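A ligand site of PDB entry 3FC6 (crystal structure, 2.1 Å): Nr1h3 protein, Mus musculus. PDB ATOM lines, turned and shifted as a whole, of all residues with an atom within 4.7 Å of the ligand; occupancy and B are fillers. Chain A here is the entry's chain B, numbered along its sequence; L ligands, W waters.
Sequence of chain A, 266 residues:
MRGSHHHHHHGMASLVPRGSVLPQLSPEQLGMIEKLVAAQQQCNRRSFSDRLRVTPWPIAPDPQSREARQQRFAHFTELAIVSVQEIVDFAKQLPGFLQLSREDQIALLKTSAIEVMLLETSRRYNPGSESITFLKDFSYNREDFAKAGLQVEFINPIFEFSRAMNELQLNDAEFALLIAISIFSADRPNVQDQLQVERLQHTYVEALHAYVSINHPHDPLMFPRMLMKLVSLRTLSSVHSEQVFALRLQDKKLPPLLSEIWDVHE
O3 of the ligand lies within hydrogen-bond range of N of Leu 135 (2.8 Å).
The side-chain amide nitrogen (ND2) of Asn 44 is in hydrogen-bond range of an oxygen (O2) of the ligand, at 2.9 Å.
An oxygen (O2) of the ligand is in salt-bridge range of the guanidinium group (NH2) of Arg 124, 3.1 Å away.
ND2 of Asn 44 lies within hydrogen-bond range of OE2 of Glu 86, 2.8 Å away.
The guanidinium group of Arg 124 lies within salt-bridge range of the side-chain carboxylate of Glu 120, at 2.6 Å.
The backbone NH of Thr 133 lies within hydrogen-bond range of the backbone carbonyl oxygen of Arg 124 (3.1 Å).
OG1 of Thr 121 sits at hydrogen-bond distance from O of Met 117 (2.7 Å).
Water W1 lies within hydrogen-bond range of O2 of the ligand (2.5 Å) and NE of Arg 124 (3.3 Å).
Water W3 lies within hydrogen-bond range of the side-chain carboxylate (OE1) of Glu 86 (2.7 Å), the side-chain carboxylate (OE1) of Glu 120 (3.4 Å) and the guanidinium group (NH2) of Arg 124 (3.5 Å).
F3 of the ligand sits close to NE2 of His 240 (3.4 Å).
O of Phe 76 touches C24 of the ligand (3.5 Å).
Leu 79 touches the ligand (O to C32, 3.2 Å).
Ala 80 touches the ligand.
Ser 83 touches the ligand (CB to C26, 3.7 Å).
OE2 of Glu 86 touches C34 of the ligand (3.8 Å).
Ile 114 touches the ligand.
Met 117 touches the ligand (CG to C13, 3.6 Å).
Leu 118 touches the ligand.
Glu 120 touches the ligand (CB to C30, 3.9 Å).
Thr 121 touches the ligand.
Ile 132 touches the ligand (CD1 to C21, 3.6 Å).
Phe 134 touches the ligand.
Phe 145 touches the ligand.
CD2 of Leu 150 touches F1 of the ligand, 3.7 Å away.
Phe 154 touches the ligand (CZ to C16, 3.7 Å).
CG1 of Ile 155 touches C19 of the ligand, 3.9 Å away.
Ile 158 touches the ligand.
Phe 159 touches the ligand (CE1 to C21, 3.6 Å).
Gln 243 touches the ligand (CG to F1, 3.6 Å).
CG2 of Val 244 touches F3 of the ligand, at 3.97 Å.
CD1 of Leu 247 touches F2 of the ligand, 3.5 Å away.
Leu 254 touches the ligand.
CZ3 of Trp 262 touches C4 of the ligand, at 3.3 Å.
Hydrophobic or aromatic side chains that line the ligand: Phe 76, Leu 79, Ile 114, Met 117, Leu 118, Ile 132, Phe 134, Leu 135, Phe 145, Leu 150, Phe 154, Ile 155, Ile 158, Phe 159, His 240, Val 244, Leu 247, Leu 254 and Trp 262.
Within 4 Å of the ligand: Asn 44, Phe 76, Leu 79, Ala 80, Ser 83, Glu 86, Ile 114, Met 117, Leu 118, Glu 120, Thr 121, Arg 124, Ile 132, Phe 134, Leu 135, Phe 145, Leu 150, Phe 154, Ile 155, Ile 158, Phe 159, His 240, Gln 243, Val 244, Leu 247, Leu 254 and Trp 262.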
ATOM      1  N   ASN A  44      14.435 -11.486  -5.644  1.00  0.00           N
ATOM      2  CA  ASN A  44      13.940 -10.120  -5.659  1.00  0.00           C
ATOM      3  C   ASN A  44      12.424 -10.024  -5.557  1.00  0.00           C
ATOM      4  O   ASN A  44      11.887  -9.042  -5.028  1.00  0.00           O
ATOM      5  CB  ASN A  44      14.425  -9.377  -6.896  1.00  0.00           C
ATOM      6  CG  ASN A  44      14.256  -7.874  -6.788  1.00  0.00           C
ATOM      7  OD1 ASN A  44      13.646  -7.245  -7.663  1.00  0.00           O
ATOM      8  ND2 ASN A  44      14.769  -7.287  -5.717  1.00  0.00           N
ATOM      9  N   PHE A  73      16.837   7.010   8.823  1.00  0.00           N
ATOM     10  CA  PHE A  73      17.905   6.045   9.059  1.00  0.00           C
ATOM     11  C   PHE A  73      17.346   4.642   9.301  1.00  0.00           C
ATOM     12  O   PHE A  73      17.930   3.641   8.862  1.00  0.00           O
ATOM     13  CB  PHE A  73      18.756   6.485  10.241  1.00  0.00           C
ATOM     14  CG  PHE A  73      19.954   5.613  10.483  1.00  0.00           C
ATOM     15  CD1 PHE A  73      19.982   4.726  11.541  1.00  0.00           C
ATOM     16  CD2 PHE A  73      21.060   5.690   9.657  1.00  0.00           C
ATOM     17  CE1 PHE A  73      21.074   3.939  11.780  1.00  0.00           C
ATOM     18  CE2 PHE A  73      22.160   4.896   9.879  1.00  0.00           C
ATOM     19  CZ  PHE A  73      22.175   4.024  10.949  1.00  0.00           C
ATOM     20  N   PHE A  76      16.293   3.344   5.947  1.00  0.00           N
ATOM     21  CA  PHE A  76      17.417   2.951   5.090  1.00  0.00           C
ATOM     22  C   PHE A  76      18.091   1.667   5.575  1.00  0.00           C
ATOM     23  O   PHE A  76      18.374   0.779   4.772  1.00  0.00           O
ATOM     24  CB  PHE A  76      18.474   4.057   4.980  1.00  0.00           C
ATOM     25  CG  PHE A  76      18.118   5.143   3.992  1.00  0.00           C
ATOM     26  CD1 PHE A  76      17.476   4.846   2.805  1.00  0.00           C
ATOM     27  CD2 PHE A  76      18.476   6.466   4.240  1.00  0.00           C
ATOM     28  CE1 PHE A  76      17.163   5.834   1.893  1.00  0.00           C
ATOM     29  CE2 PHE A  76      18.164   7.471   3.332  1.00  0.00           C
ATOM     30  CZ  PHE A  76      17.506   7.155   2.170  1.00  0.00           C
ATOM     31  N   THR A  77      18.348   1.576   6.868  1.00  0.00           N
ATOM     32  CA  THR A  77      18.927   0.361   7.433  1.00  0.00           C
ATOM     33  C   THR A  77      17.996  -0.853   7.269  1.00  0.00           C
ATOM     34  O   THR A  77      18.451  -1.985   7.150  1.00  0.00           O
ATOM     35  CB  THR A  77      19.305   0.536   8.911  1.00  0.00           C
ATOM     36  OG1 THR A  77      18.157   0.950   9.665  1.00  0.00           O
ATOM     37  CG2 THR A  77      20.403   1.594   9.065  1.00  0.00           C
ATOM     38  N   LEU A  79      15.843  -1.251   4.688  1.00  0.00           N
ATOM     39  CA  LEU A  79      16.026  -1.607   3.284  1.00  0.00           C
ATOM     40  C   LEU A  79      17.269  -2.469   3.103  1.00  0.00           C
ATOM     41  O   LEU A  79      17.236  -3.493   2.420  1.00  0.00           O
ATOM     42  CB  LEU A  79      16.140  -0.360   2.413  1.00  0.00           C
ATOM     43  CG  LEU A  79      14.877   0.444   2.184  1.00  0.00           C
ATOM     44  CD1 LEU A  79      15.181   1.639   1.256  1.00  0.00           C
ATOM     45  CD2 LEU A  79      13.826  -0.455   1.566  1.00  0.00           C
ATOM     46  N   ALA A  80      18.367  -2.037   3.726  1.00  0.00           N
ATOM     47  CA  ALA A  80      19.627  -2.776   3.687  1.00  0.00           C
ATOM     48  C   ALA A  80      19.462  -4.231   4.130  1.00  0.00           C
ATOM     49  O   ALA A  80      20.054  -5.143   3.561  1.00  0.00           O
ATOM     50  CB  ALA A  80      20.665  -2.094   4.562  1.00  0.00           C
ATOM     51  N   VAL A  82      16.825  -6.046   3.939  1.00  0.00           N
ATOM     52  CA  VAL A  82      16.161  -6.750   2.863  1.00  0.00           C
ATOM     53  C   VAL A  82      17.222  -7.134   1.820  1.00  0.00           C
ATOM     54  O   VAL A  82      17.243  -8.256   1.299  1.00  0.00           O
ATOM     55  CB  VAL A  82      15.033  -5.901   2.261  1.00  0.00           C
ATOM     56  CG1 VAL A  82      14.469  -6.535   1.010  1.00  0.00           C
ATOM     57  CG2 VAL A  82      13.931  -5.694   3.317  1.00  0.00           C
ATOM     58  N   SER A  83      18.126  -6.195   1.537  1.00  0.00           N
ATOM     59  CA  SER A  83      19.181  -6.465   0.583  1.00  0.00           C
ATOM     60  C   SER A  83      20.030  -7.656   1.022  1.00  0.00           C
ATOM     61  O   SER A  83      20.301  -8.546   0.226  1.00  0.00           O
ATOM     62  CB  SER A  83      20.069  -5.237   0.401  1.00  0.00           C
ATOM     63  OG  SER A  83      21.016  -5.474  -0.629  1.00  0.00           O
ATOM     64  N   GLU A  86      18.239 -10.854   0.537  1.00  0.00           N
ATOM     65  CA  GLU A  86      18.239 -11.244  -0.864  1.00  0.00           C
ATOM     66  C   GLU A  86      19.597 -11.812  -1.278  1.00  0.00           C
ATOM     67  O   GLU A  86      19.685 -12.805  -2.015  1.00  0.00           O
ATOM     68  CB  GLU A  86      17.825 -10.057  -1.757  1.00  0.00           C
ATOM     69  CG  GLU A  86      17.652 -10.433  -3.207  1.00  0.00           C
ATOM     70  CD  GLU A  86      17.202  -9.268  -4.082  1.00  0.00           C
ATOM     71  OE1 GLU A  86      17.797  -9.081  -5.163  1.00  0.00           O
ATOM     72  OE2 GLU A  86      16.251  -8.555  -3.715  1.00  0.00           O
ATOM     73  N   ILE A 114      28.428  -5.947   1.314  1.00  0.00           N
ATOM     74  CA  ILE A 114      28.457  -4.541   0.949  1.00  0.00           C
ATOM     75  C   ILE A 114      28.741  -4.357  -0.555  1.00  0.00           C
ATOM     76  O   ILE A 114      28.192  -3.441  -1.187  1.00  0.00           O
ATOM     77  CB  ILE A 114      29.442  -3.724   1.811  1.00  0.00           C
ATOM     78  CG1 ILE A 114      29.197  -2.235   1.595  1.00  0.00           C
ATOM     79  CG2 ILE A 114      30.894  -4.115   1.515  1.00  0.00           C
ATOM     80  CD1 ILE A 114      27.869  -1.765   2.171  1.00  0.00           C
ATOM     81  N   MET A 117      25.632  -5.346  -2.547  1.00  0.00           N
ATOM     82  CA  MET A 117      24.650  -4.310  -2.291  1.00  0.00           C
ATOM     83  C   MET A 117      24.976  -3.085  -3.174  1.00  0.00           C
ATOM     84  O   MET A 117      24.076  -2.419  -3.664  1.00  0.00           O
ATOM     85  CB  MET A 117      24.617  -3.943  -0.800  1.00  0.00           C
ATOM     86  CG  MET A 117      23.374  -3.177  -0.352  1.00  0.00           C
ATOM     87  SD  MET A 117      23.326  -2.877   1.458  1.00  0.00           S
ATOM     88  CE  MET A 117      24.058  -4.399   1.981  1.00  0.00           C
ATOM     89  N   LEU A 118      26.261  -2.818  -3.377  1.00  0.00           N
ATOM     90  CA  LEU A 118      26.687  -1.682  -4.199  1.00  0.00           C
ATOM     91  C   LEU A 118      26.374  -1.917  -5.680  1.00  0.00           C
ATOM     92  O   LEU A 118      25.865  -1.012  -6.360  1.00  0.00           O
ATOM     93  CB  LEU A 118      28.176  -1.406  -4.018  1.00  0.00           C
ATOM     94  CG  LEU A 118      28.519  -0.565  -2.793  1.00  0.00           C
ATOM     95  CD1 LEU A 118      30.007  -0.658  -2.483  1.00  0.00           C
ATOM     96  CD2 LEU A 118      28.091   0.885  -2.992  1.00  0.00           C
ATOM     97  N   GLU A 120      24.021  -4.008  -6.840  1.00  0.00           N
ATOM     98  CA  GLU A 120      22.559  -3.938  -6.974  1.00  0.00           C
ATOM     99  C   GLU A 120      22.060  -2.502  -6.963  1.00  0.00           C
ATOM    100  O   GLU A 120      21.084  -2.169  -7.634  1.00  0.00           O
ATOM    101  CB  GLU A 120      21.877  -4.757  -5.876  1.00  0.00           C
ATOM    102  CG  GLU A 120      22.013  -6.256  -6.106  1.00  0.00           C
ATOM    103  CD  GLU A 120      21.375  -6.677  -7.414  1.00  0.00           C
ATOM    104  OE1 GLU A 120      20.415  -6.023  -7.854  1.00  0.00           O
ATOM    105  OE2 GLU A 120      21.827  -7.663  -8.014  1.00  0.00           O
ATOM    106  N   THR A 121      22.740  -1.661  -6.202  1.00  0.00           N
ATOM    107  CA  THR A 121      22.382  -0.252  -6.114  1.00  0.00           C
ATOM    108  C   THR A 121      22.644   0.481  -7.435  1.00  0.00           C
ATOM    109  O   THR A 121      21.836   1.305  -7.871  1.00  0.00           O
ATOM    110  CB  THR A 121      23.151   0.426  -4.968  1.00  0.00           C
ATOM    111  OG1 THR A 121      22.662  -0.082  -3.720  1.00  0.00           O
ATOM    112  CG2 THR A 121      22.990   1.967  -5.005  1.00  0.00           C
ATOM    113  N   ARG A 124      20.129   0.341  -9.987  1.00  0.00           N
ATOM    114  CA  ARG A 124      18.871   1.035  -9.762  1.00  0.00           C
ATOM    115  C   ARG A 124      19.062   2.554  -9.772  1.00  0.00           C
ATOM    116  O   ARG A 124      18.226   3.302  -9.275  1.00  0.00           O
ATOM    117  CB  ARG A 124      18.246   0.552  -8.444  1.00  0.00           C
ATOM    118  CG  ARG A 124      17.841  -0.925  -8.490  1.00  0.00           C
ATOM    119  CD  ARG A 124      17.511  -1.528  -7.140  1.00  0.00           C
ATOM    120  NE  ARG A 124      16.900  -2.851  -7.240  1.00  0.00           N
ATOM    121  CZ  ARG A 124      17.575  -3.964  -7.530  1.00  0.00           C
ATOM    122  NH1 ARG A 124      18.887  -3.916  -7.741  1.00  0.00           N
ATOM    123  NH2 ARG A 124      16.949  -5.131  -7.588  1.00  0.00           N
ATOM    124  N   ILE A 132      18.172   7.024  -6.872  1.00  0.00           N
ATOM    125  CA  ILE A 132      18.233   5.579  -6.769  1.00  0.00           C
ATOM    126  C   ILE A 132      16.875   5.068  -6.278  1.00  0.00           C
ATOM    127  O   ILE A 132      16.305   5.614  -5.345  1.00  0.00           O
ATOM    128  CB  ILE A 132      19.353   5.150  -5.813  1.00  0.00           C
ATOM    129  CG1 ILE A 132      20.693   5.658  -6.334  1.00  0.00           C
ATOM    130  CG2 ILE A 132      19.399   3.647  -5.667  1.00  0.00           C
ATOM    131  CD1 ILE A 132      21.819   5.534  -5.333  1.00  0.00           C
ATOM    132  N   THR A 133      16.361   4.030  -6.935  1.00  0.00           N
ATOM    133  CA  THR A 133      15.040   3.533  -6.588  1.00  0.00           C
ATOM    134  C   THR A 133      15.131   2.115  -6.069  1.00  0.00           C
ATOM    135  O   THR A 133      15.650   1.228  -6.755  1.00  0.00           O
ATOM    136  CB  THR A 133      14.091   3.548  -7.792  1.00  0.00           C
ATOM    137  OG1 THR A 133      14.052   4.862  -8.347  1.00  0.00           O
ATOM    138  CG2 THR A 133      12.690   3.132  -7.362  1.00  0.00           C
ATOM    139  N   PHE A 134      14.646   1.913  -4.849  1.00  0.00           N
ATOM    140  CA  PHE A 134      14.592   0.584  -4.258  1.00  0.00           C
ATOM    141  C   PHE A 134      13.175   0.083  -4.224  1.00  0.00           C
ATOM    142  O   PHE A 134      12.240   0.856  -3.995  1.00  0.00           O
ATOM    143  CB  PHE A 134      15.131   0.623  -2.836  1.00  0.00           C
ATOM    144  CG  PHE A 134      16.492   1.211  -2.721  1.00  0.00           C
ATOM    145  CD1 PHE A 134      17.610   0.489  -3.103  1.00  0.00           C
ATOM    146  CD2 PHE A 134      16.666   2.498  -2.221  1.00  0.00           C
ATOM    147  CE1 PHE A 134      18.877   1.036  -2.988  1.00  0.00           C
ATOM    148  CE2 PHE A 134      17.921   3.044  -2.099  1.00  0.00           C
ATOM    149  CZ  PHE A 134      19.031   2.316  -2.482  1.00  0.00           C
ATOM    150  N   LEU A 135      13.017  -1.214  -4.463  1.00  0.00           N
ATOM    151  CA  LEU A 135      11.710  -1.863  -4.421  1.00  0.00           C
ATOM    152  C   LEU A 135      10.623  -1.082  -5.152  1.00  0.00           C
ATOM    153  O   LEU A 135       9.464  -1.099  -4.732  1.00  0.00           O
ATOM    154  CB  LEU A 135      11.290  -2.121  -2.968  1.00  0.00           C
ATOM    155  CG  LEU A 135      12.230  -3.050  -2.213  1.00  0.00           C
ATOM    156  CD1 LEU A 135      11.852  -3.089  -0.733  1.00  0.00           C
ATOM    157  CD2 LEU A 135      12.257  -4.464  -2.827  1.00  0.00           C
ATOM    158  N   PHE A 145      19.626  10.992   1.146  1.00  0.00           N
ATOM    159  CA  PHE A 145      20.532  10.182   1.926  1.00  0.00           C
ATOM    160  C   PHE A 145      21.213  11.017   3.022  1.00  0.00           C
ATOM    161  O   PHE A 145      21.480  10.507   4.115  1.00  0.00           O
ATOM    162  CB  PHE A 145      21.564   9.479   1.047  1.00  0.00           C
ATOM    163  CG  PHE A 145      20.974   8.412   0.143  1.00  0.00           C
ATOM    164  CD1 PHE A 145      20.692   7.154   0.635  1.00  0.00           C
ATOM    165  CD2 PHE A 145      20.711   8.684  -1.197  1.00  0.00           C
ATOM    166  CE1 PHE A 145      20.141   6.175  -0.195  1.00  0.00           C
ATOM    167  CE2 PHE A 145      20.176   7.715  -2.025  1.00  0.00           C
ATOM    168  CZ  PHE A 145      19.891   6.461  -1.525  1.00  0.00           C
ATOM    169  N   LEU A 150      23.801  10.431   6.747  1.00  0.00           N
ATOM    170  CA  LEU A 150      24.942   9.835   6.046  1.00  0.00           C
ATOM    171  C   LEU A 150      25.877  10.947   5.583  1.00  0.00           C
ATOM    172  O   LEU A 150      25.425  12.010   5.178  1.00  0.00           O
ATOM    173  CB  LEU A 150      24.465   8.985   4.860  1.00  0.00           C
ATOM    174  CG  LEU A 150      23.670   7.737   5.247  1.00  0.00           C
ATOM    175  CD1 LEU A 150      23.156   6.988   4.022  1.00  0.00           C
ATOM    176  CD2 LEU A 150      24.532   6.831   6.098  1.00  0.00           C
ATOM    177  N   PHE A 154      30.649   9.307   2.001  1.00  0.00           N
ATOM    178  CA  PHE A 154      30.010   8.016   1.778  1.00  0.00           C
ATOM    179  C   PHE A 154      29.078   8.171   0.567  1.00  0.00           C
ATOM    180  O   PHE A 154      29.136   7.398  -0.389  1.00  0.00           O
ATOM    181  CB  PHE A 154      29.203   7.624   3.009  1.00  0.00           C
ATOM    182  CG  PHE A 154      28.577   6.242   2.952  1.00  0.00           C
ATOM    183  CD1 PHE A 154      29.351   5.114   2.714  1.00  0.00           C
ATOM    184  CD2 PHE A 154      27.233   6.083   3.222  1.00  0.00           C
ATOM    185  CE1 PHE A 154      28.772   3.849   2.708  1.00  0.00           C
ATOM    186  CE2 PHE A 154      26.638   4.823   3.218  1.00  0.00           C
ATOM    187  CZ  PHE A 154      27.424   3.700   2.959  1.00  0.00           C
ATOM    188  N   ILE A 155      28.244   9.196   0.611  1.00  0.00           N
ATOM    189  CA  ILE A 155      27.280   9.420  -0.457  1.00  0.00           C
ATOM    190  C   ILE A 155      27.902   9.635  -1.846  1.00  0.00           C
ATOM    191  O   ILE A 155      27.568   8.937  -2.799  1.00  0.00           O
ATOM    192  CB  ILE A 155      26.342  10.586  -0.108  1.00  0.00           C
ATOM    193  CG1 ILE A 155      25.430  10.199   1.061  1.00  0.00           C
ATOM    194  CG2 ILE A 155      25.500  10.963  -1.307  1.00  0.00           C
ATOM    195  CD1 ILE A 155      24.723  11.405   1.721  1.00  0.00           C
ATOM    196  N   ILE A 158      29.534   6.698  -3.781  1.00  0.00           N
ATOM    197  CA  ILE A 158      28.546   5.716  -4.204  1.00  0.00           C
ATOM    198  C   ILE A 158      27.725   6.204  -5.395  1.00  0.00           C
ATOM    199  O   ILE A 158      27.389   5.425  -6.289  1.00  0.00           O
ATOM    200  CB  ILE A 158      27.617   5.272  -3.063  1.00  0.00           C
ATOM    201  CG1 ILE A 158      28.443   4.599  -1.965  1.00  0.00           C
ATOM    202  CG2 ILE A 158      26.565   4.300  -3.591  1.00  0.00           C
ATOM    203  CD1 ILE A 158      27.666   4.421  -0.686  1.00  0.00           C
ATOM    204  N   PHE A 159      27.409   7.488  -5.423  1.00  0.00           N
ATOM    205  CA  PHE A 159      26.740   8.036  -6.595  1.00  0.00           C
ATOM    206  C   PHE A 159      27.657   7.991  -7.807  1.00  0.00           C
ATOM    207  O   PHE A 159      27.209   7.692  -8.906  1.00  0.00           O
ATOM    208  CB  PHE A 159      26.179   9.440  -6.349  1.00  0.00           C
ATOM    209  CG  PHE A 159      24.760   9.436  -5.874  1.00  0.00           C
ATOM    210  CD1 PHE A 159      24.463   9.203  -4.543  1.00  0.00           C
ATOM    211  CD2 PHE A 159      23.711   9.618  -6.759  1.00  0.00           C
ATOM    212  CE1 PHE A 159      23.170   9.182  -4.098  1.00  0.00           C
ATOM    213  CE2 PHE A 159      22.406   9.598  -6.321  1.00  0.00           C
ATOM    214  CZ  PHE A 159      22.133   9.382  -4.987  1.00  0.00           C
ATOM    215  N   HIS A 240      32.757   2.576   3.130  1.00  0.00           N
ATOM    216  CA  HIS A 240      31.633   2.121   3.915  1.00  0.00           C
ATOM    217  C   HIS A 240      32.042   1.915   5.363  1.00  0.00           C
ATOM    218  O   HIS A 240      31.332   2.329   6.279  1.00  0.00           O
ATOM    219  CB  HIS A 240      31.068   0.820   3.328  1.00  0.00           C
ATOM    220  CG  HIS A 240      30.107   0.118   4.224  1.00  0.00           C
ATOM    221  ND1 HIS A 240      30.384  -1.105   4.811  1.00  0.00           N
ATOM    222  CD2 HIS A 240      28.884   0.474   4.687  1.00  0.00           C
ATOM    223  CE1 HIS A 240      29.365  -1.473   5.557  1.00  0.00           C
ATOM    224  NE2 HIS A 240      28.443  -0.531   5.516  1.00  0.00           N
ATOM    225  N   GLN A 243      32.138   5.050   7.136  1.00  0.00           N
ATOM    226  CA  GLN A 243      30.804   5.556   7.422  1.00  0.00           C
ATOM    227  C   GLN A 243      30.232   4.821   8.628  1.00  0.00           C
ATOM    228  O   GLN A 243      29.570   5.432   9.478  1.00  0.00           O
ATOM    229  CB  GLN A 243      29.883   5.385   6.219  1.00  0.00           C
ATOM    230  CG  GLN A 243      28.418   5.582   6.500  1.00  0.00           C
ATOM    231  CD  GLN A 243      28.081   7.011   6.849  1.00  0.00           C
ATOM    232  OE1 GLN A 243      27.676   7.803   5.982  1.00  0.00           O
ATOM    233  NE2 GLN A 243      28.237   7.362   8.124  1.00  0.00           N
ATOM    234  N   VAL A 244      30.489   3.521   8.719  1.00  0.00           N
ATOM    235  CA  VAL A 244      30.034   2.768   9.879  1.00  0.00           C
ATOM    236  C   VAL A 244      30.554   3.424  11.159  1.00  0.00           C
ATOM    237  O   VAL A 244      29.774   3.789  12.042  1.00  0.00           O
ATOM    238  CB  VAL A 244      30.494   1.294   9.807  1.00  0.00           C
ATOM    239  CG1 VAL A 244      30.228   0.599  11.145  1.00  0.00           C
ATOM    240  CG2 VAL A 244      29.779   0.585   8.687  1.00  0.00           C
ATOM    241  N   LEU A 247      28.971   6.706  12.027  1.00  0.00           N
ATOM    242  CA  LEU A 247      27.663   6.464  12.669  1.00  0.00           C
ATOM    243  C   LEU A 247      27.768   6.242  14.188  1.00  0.00           C
ATOM    244  O   LEU A 247      26.923   6.712  14.948  1.00  0.00           O
ATOM    245  CB  LEU A 247      26.971   5.256  12.030  1.00  0.00           C
ATOM    246  CG  LEU A 247      26.460   5.462  10.608  1.00  0.00           C
ATOM    247  CD1 LEU A 247      25.780   4.206  10.102  1.00  0.00           C
ATOM    248  CD2 LEU A 247      25.510   6.639  10.578  1.00  0.00           C
ATOM    249  N   LEU A 254      23.274   0.435  14.451  1.00  0.00           N
ATOM    250  CA  LEU A 254      22.875  -0.443  13.371  1.00  0.00           C
ATOM    251  C   LEU A 254      22.019  -1.585  13.920  1.00  0.00           C
ATOM    252  O   LEU A 254      22.250  -2.046  15.034  1.00  0.00           O
ATOM    253  CB  LEU A 254      24.109  -1.032  12.663  1.00  0.00           C
ATOM    254  CG  LEU A 254      24.987  -0.108  11.807  1.00  0.00           C
ATOM    255  CD1 LEU A 254      26.143  -0.900  11.237  1.00  0.00           C
ATOM    256  CD2 LEU A 254      24.177   0.530  10.684  1.00  0.00           C
ATOM    257  N   TRP A 262      28.985  -5.899  10.126  1.00  0.00           N
ATOM    258  CA  TRP A 262      29.809  -4.704   9.871  1.00  0.00           C
ATOM    259  C   TRP A 262      30.466  -4.042  11.104  1.00  0.00           C
ATOM    260  O   TRP A 262      31.604  -3.601  11.019  1.00  0.00           O
ATOM    261  CB  TRP A 262      29.019  -3.642   9.125  1.00  0.00           C
ATOM    262  CG  TRP A 262      28.559  -4.046   7.772  1.00  0.00           C
ATOM    263  CD1 TRP A 262      29.139  -4.952   6.933  1.00  0.00           C
ATOM    264  CD2 TRP A 262      27.411  -3.527   7.082  1.00  0.00           C
ATOM    265  NE1 TRP A 262      28.411  -5.035   5.754  1.00  0.00           N
ATOM    266  CE2 TRP A 262      27.350  -4.167   5.836  1.00  0.00           C
ATOM    267  CE3 TRP A 262      26.431  -2.580   7.403  1.00  0.00           C
ATOM    268  CZ2 TRP A 262      26.345  -3.897   4.907  1.00  0.00           C
ATOM    269  CZ3 TRP A 262      25.443  -2.318   6.485  1.00  0.00           C
ATOM    270  CH2 TRP A 262      25.406  -2.963   5.252  1.00  0.00           C
HETATM  271  F1  LIG L   1      25.569   3.321   6.577  1.00  0.00           F
HETATM  272  C1  LIG L   1      25.161   2.092   6.810  1.00  0.00           C
HETATM  273  F2  LIG L   1      24.260   2.145   7.789  1.00  0.00           F
HETATM  274  F3  LIG L   1      26.184   1.373   7.201  1.00  0.00           F
HETATM  275  C2  LIG L   1      24.580   1.525   5.534  1.00  0.00           C
HETATM  276  C3  LIG L   1      23.290   2.034   5.021  1.00  0.00           C
HETATM  277 CL1  LIG L   1      22.470   3.284   5.989  1.00  0.00          CL
HETATM  278  C4  LIG L   1      25.233   0.560   4.801  1.00  0.00           C
HETATM  279  C5  LIG L   1      24.651   0.099   3.620  1.00  0.00           C
HETATM  280  C6  LIG L   1      23.432   0.571   3.132  1.00  0.00           C
HETATM  281  C7  LIG L   1      22.737   1.549   3.840  1.00  0.00           C
HETATM  282  C8  LIG L   1      21.411   2.060   3.322  1.00  0.00           C
HETATM  283  N1  LIG L   1      21.411   2.306   1.886  1.00  0.00           N
HETATM  284  C9  LIG L   1      22.213   3.450   1.443  1.00  0.00           C
HETATM  285  C10 LIG L   1      22.689   3.266  -0.013  1.00  0.00           C
HETATM  286  C11 LIG L   1      23.713   2.188  -0.113  1.00  0.00           C
HETATM  287  C12 LIG L   1      23.554   1.172  -1.046  1.00  0.00           C
HETATM  288  C13 LIG L   1      24.517   0.167  -1.147  1.00  0.00           C
HETATM  289  C14 LIG L   1      25.634   0.185  -0.320  1.00  0.00           C
HETATM  290  C15 LIG L   1      25.796   1.214   0.609  1.00  0.00           C
HETATM  291  C16 LIG L   1      24.845   2.221   0.703  1.00  0.00           C
HETATM  292  C17 LIG L   1      23.261   4.561  -0.497  1.00  0.00           C
HETATM  293  C18 LIG L   1      23.854   5.446   0.395  1.00  0.00           C
HETATM  294  C19 LIG L   1      24.374   6.663  -0.042  1.00  0.00           C
HETATM  295  C20 LIG L   1      24.288   7.017  -1.388  1.00  0.00           C
HETATM  296  C21 LIG L   1      23.694   6.132  -2.280  1.00  0.00           C
HETATM  297  C22 LIG L   1      23.174   4.915  -1.842  1.00  0.00           C
HETATM  298  C23 LIG L   1      20.112   2.193   1.245  1.00  0.00           C
HETATM  299  C24 LIG L   1      19.576   0.780   1.454  1.00  0.00           C
HETATM  300  C25 LIG L   1      19.577   0.068   0.114  1.00  0.00           C
HETATM  301  O1  LIG L   1      19.139  -1.288   0.153  1.00  0.00           O
HETATM  302  C26 LIG L   1      19.116  -1.982  -1.028  1.00  0.00           C
HETATM  303  C27 LIG L   1      17.983  -2.686  -1.415  1.00  0.00           C
HETATM  304  C28 LIG L   1      17.892  -3.391  -2.575  1.00  0.00           C
HETATM  305  C29 LIG L   1      19.045  -3.393  -3.439  1.00  0.00           C
HETATM  306  C30 LIG L   1      20.194  -2.692  -3.067  1.00  0.00           C
HETATM  307  C31 LIG L   1      20.225  -1.979  -1.867  1.00  0.00           C
HETATM  308  C32 LIG L   1      16.814  -2.776  -0.671  1.00  0.00           C
HETATM  309  C33 LIG L   1      16.002  -3.575  -1.475  1.00  0.00           C
HETATM  310  N2  LIG L   1      16.664  -3.945  -2.597  1.00  0.00           N
HETATM  311  C34 LIG L   1      16.114  -4.783  -3.668  1.00  0.00           C
HETATM  312  C35 LIG L   1      15.396  -3.868  -4.625  1.00  0.00           C
HETATM  313  O2  LIG L   1      14.772  -4.374  -5.568  1.00  0.00           O
HETATM  314  O3  LIG L   1      15.454  -2.631  -4.427  1.00  0.00           O
HETATM  315  O   HOH W   1      13.643  -3.190  -7.516  1.00  0.00           O
HETATM  316  O   HOH W   2      20.521  -6.529  -3.035  1.00  0.00           O
HETATM  317  O   HOH W   3      18.696  -6.521  -4.938  1.00  0.00           O
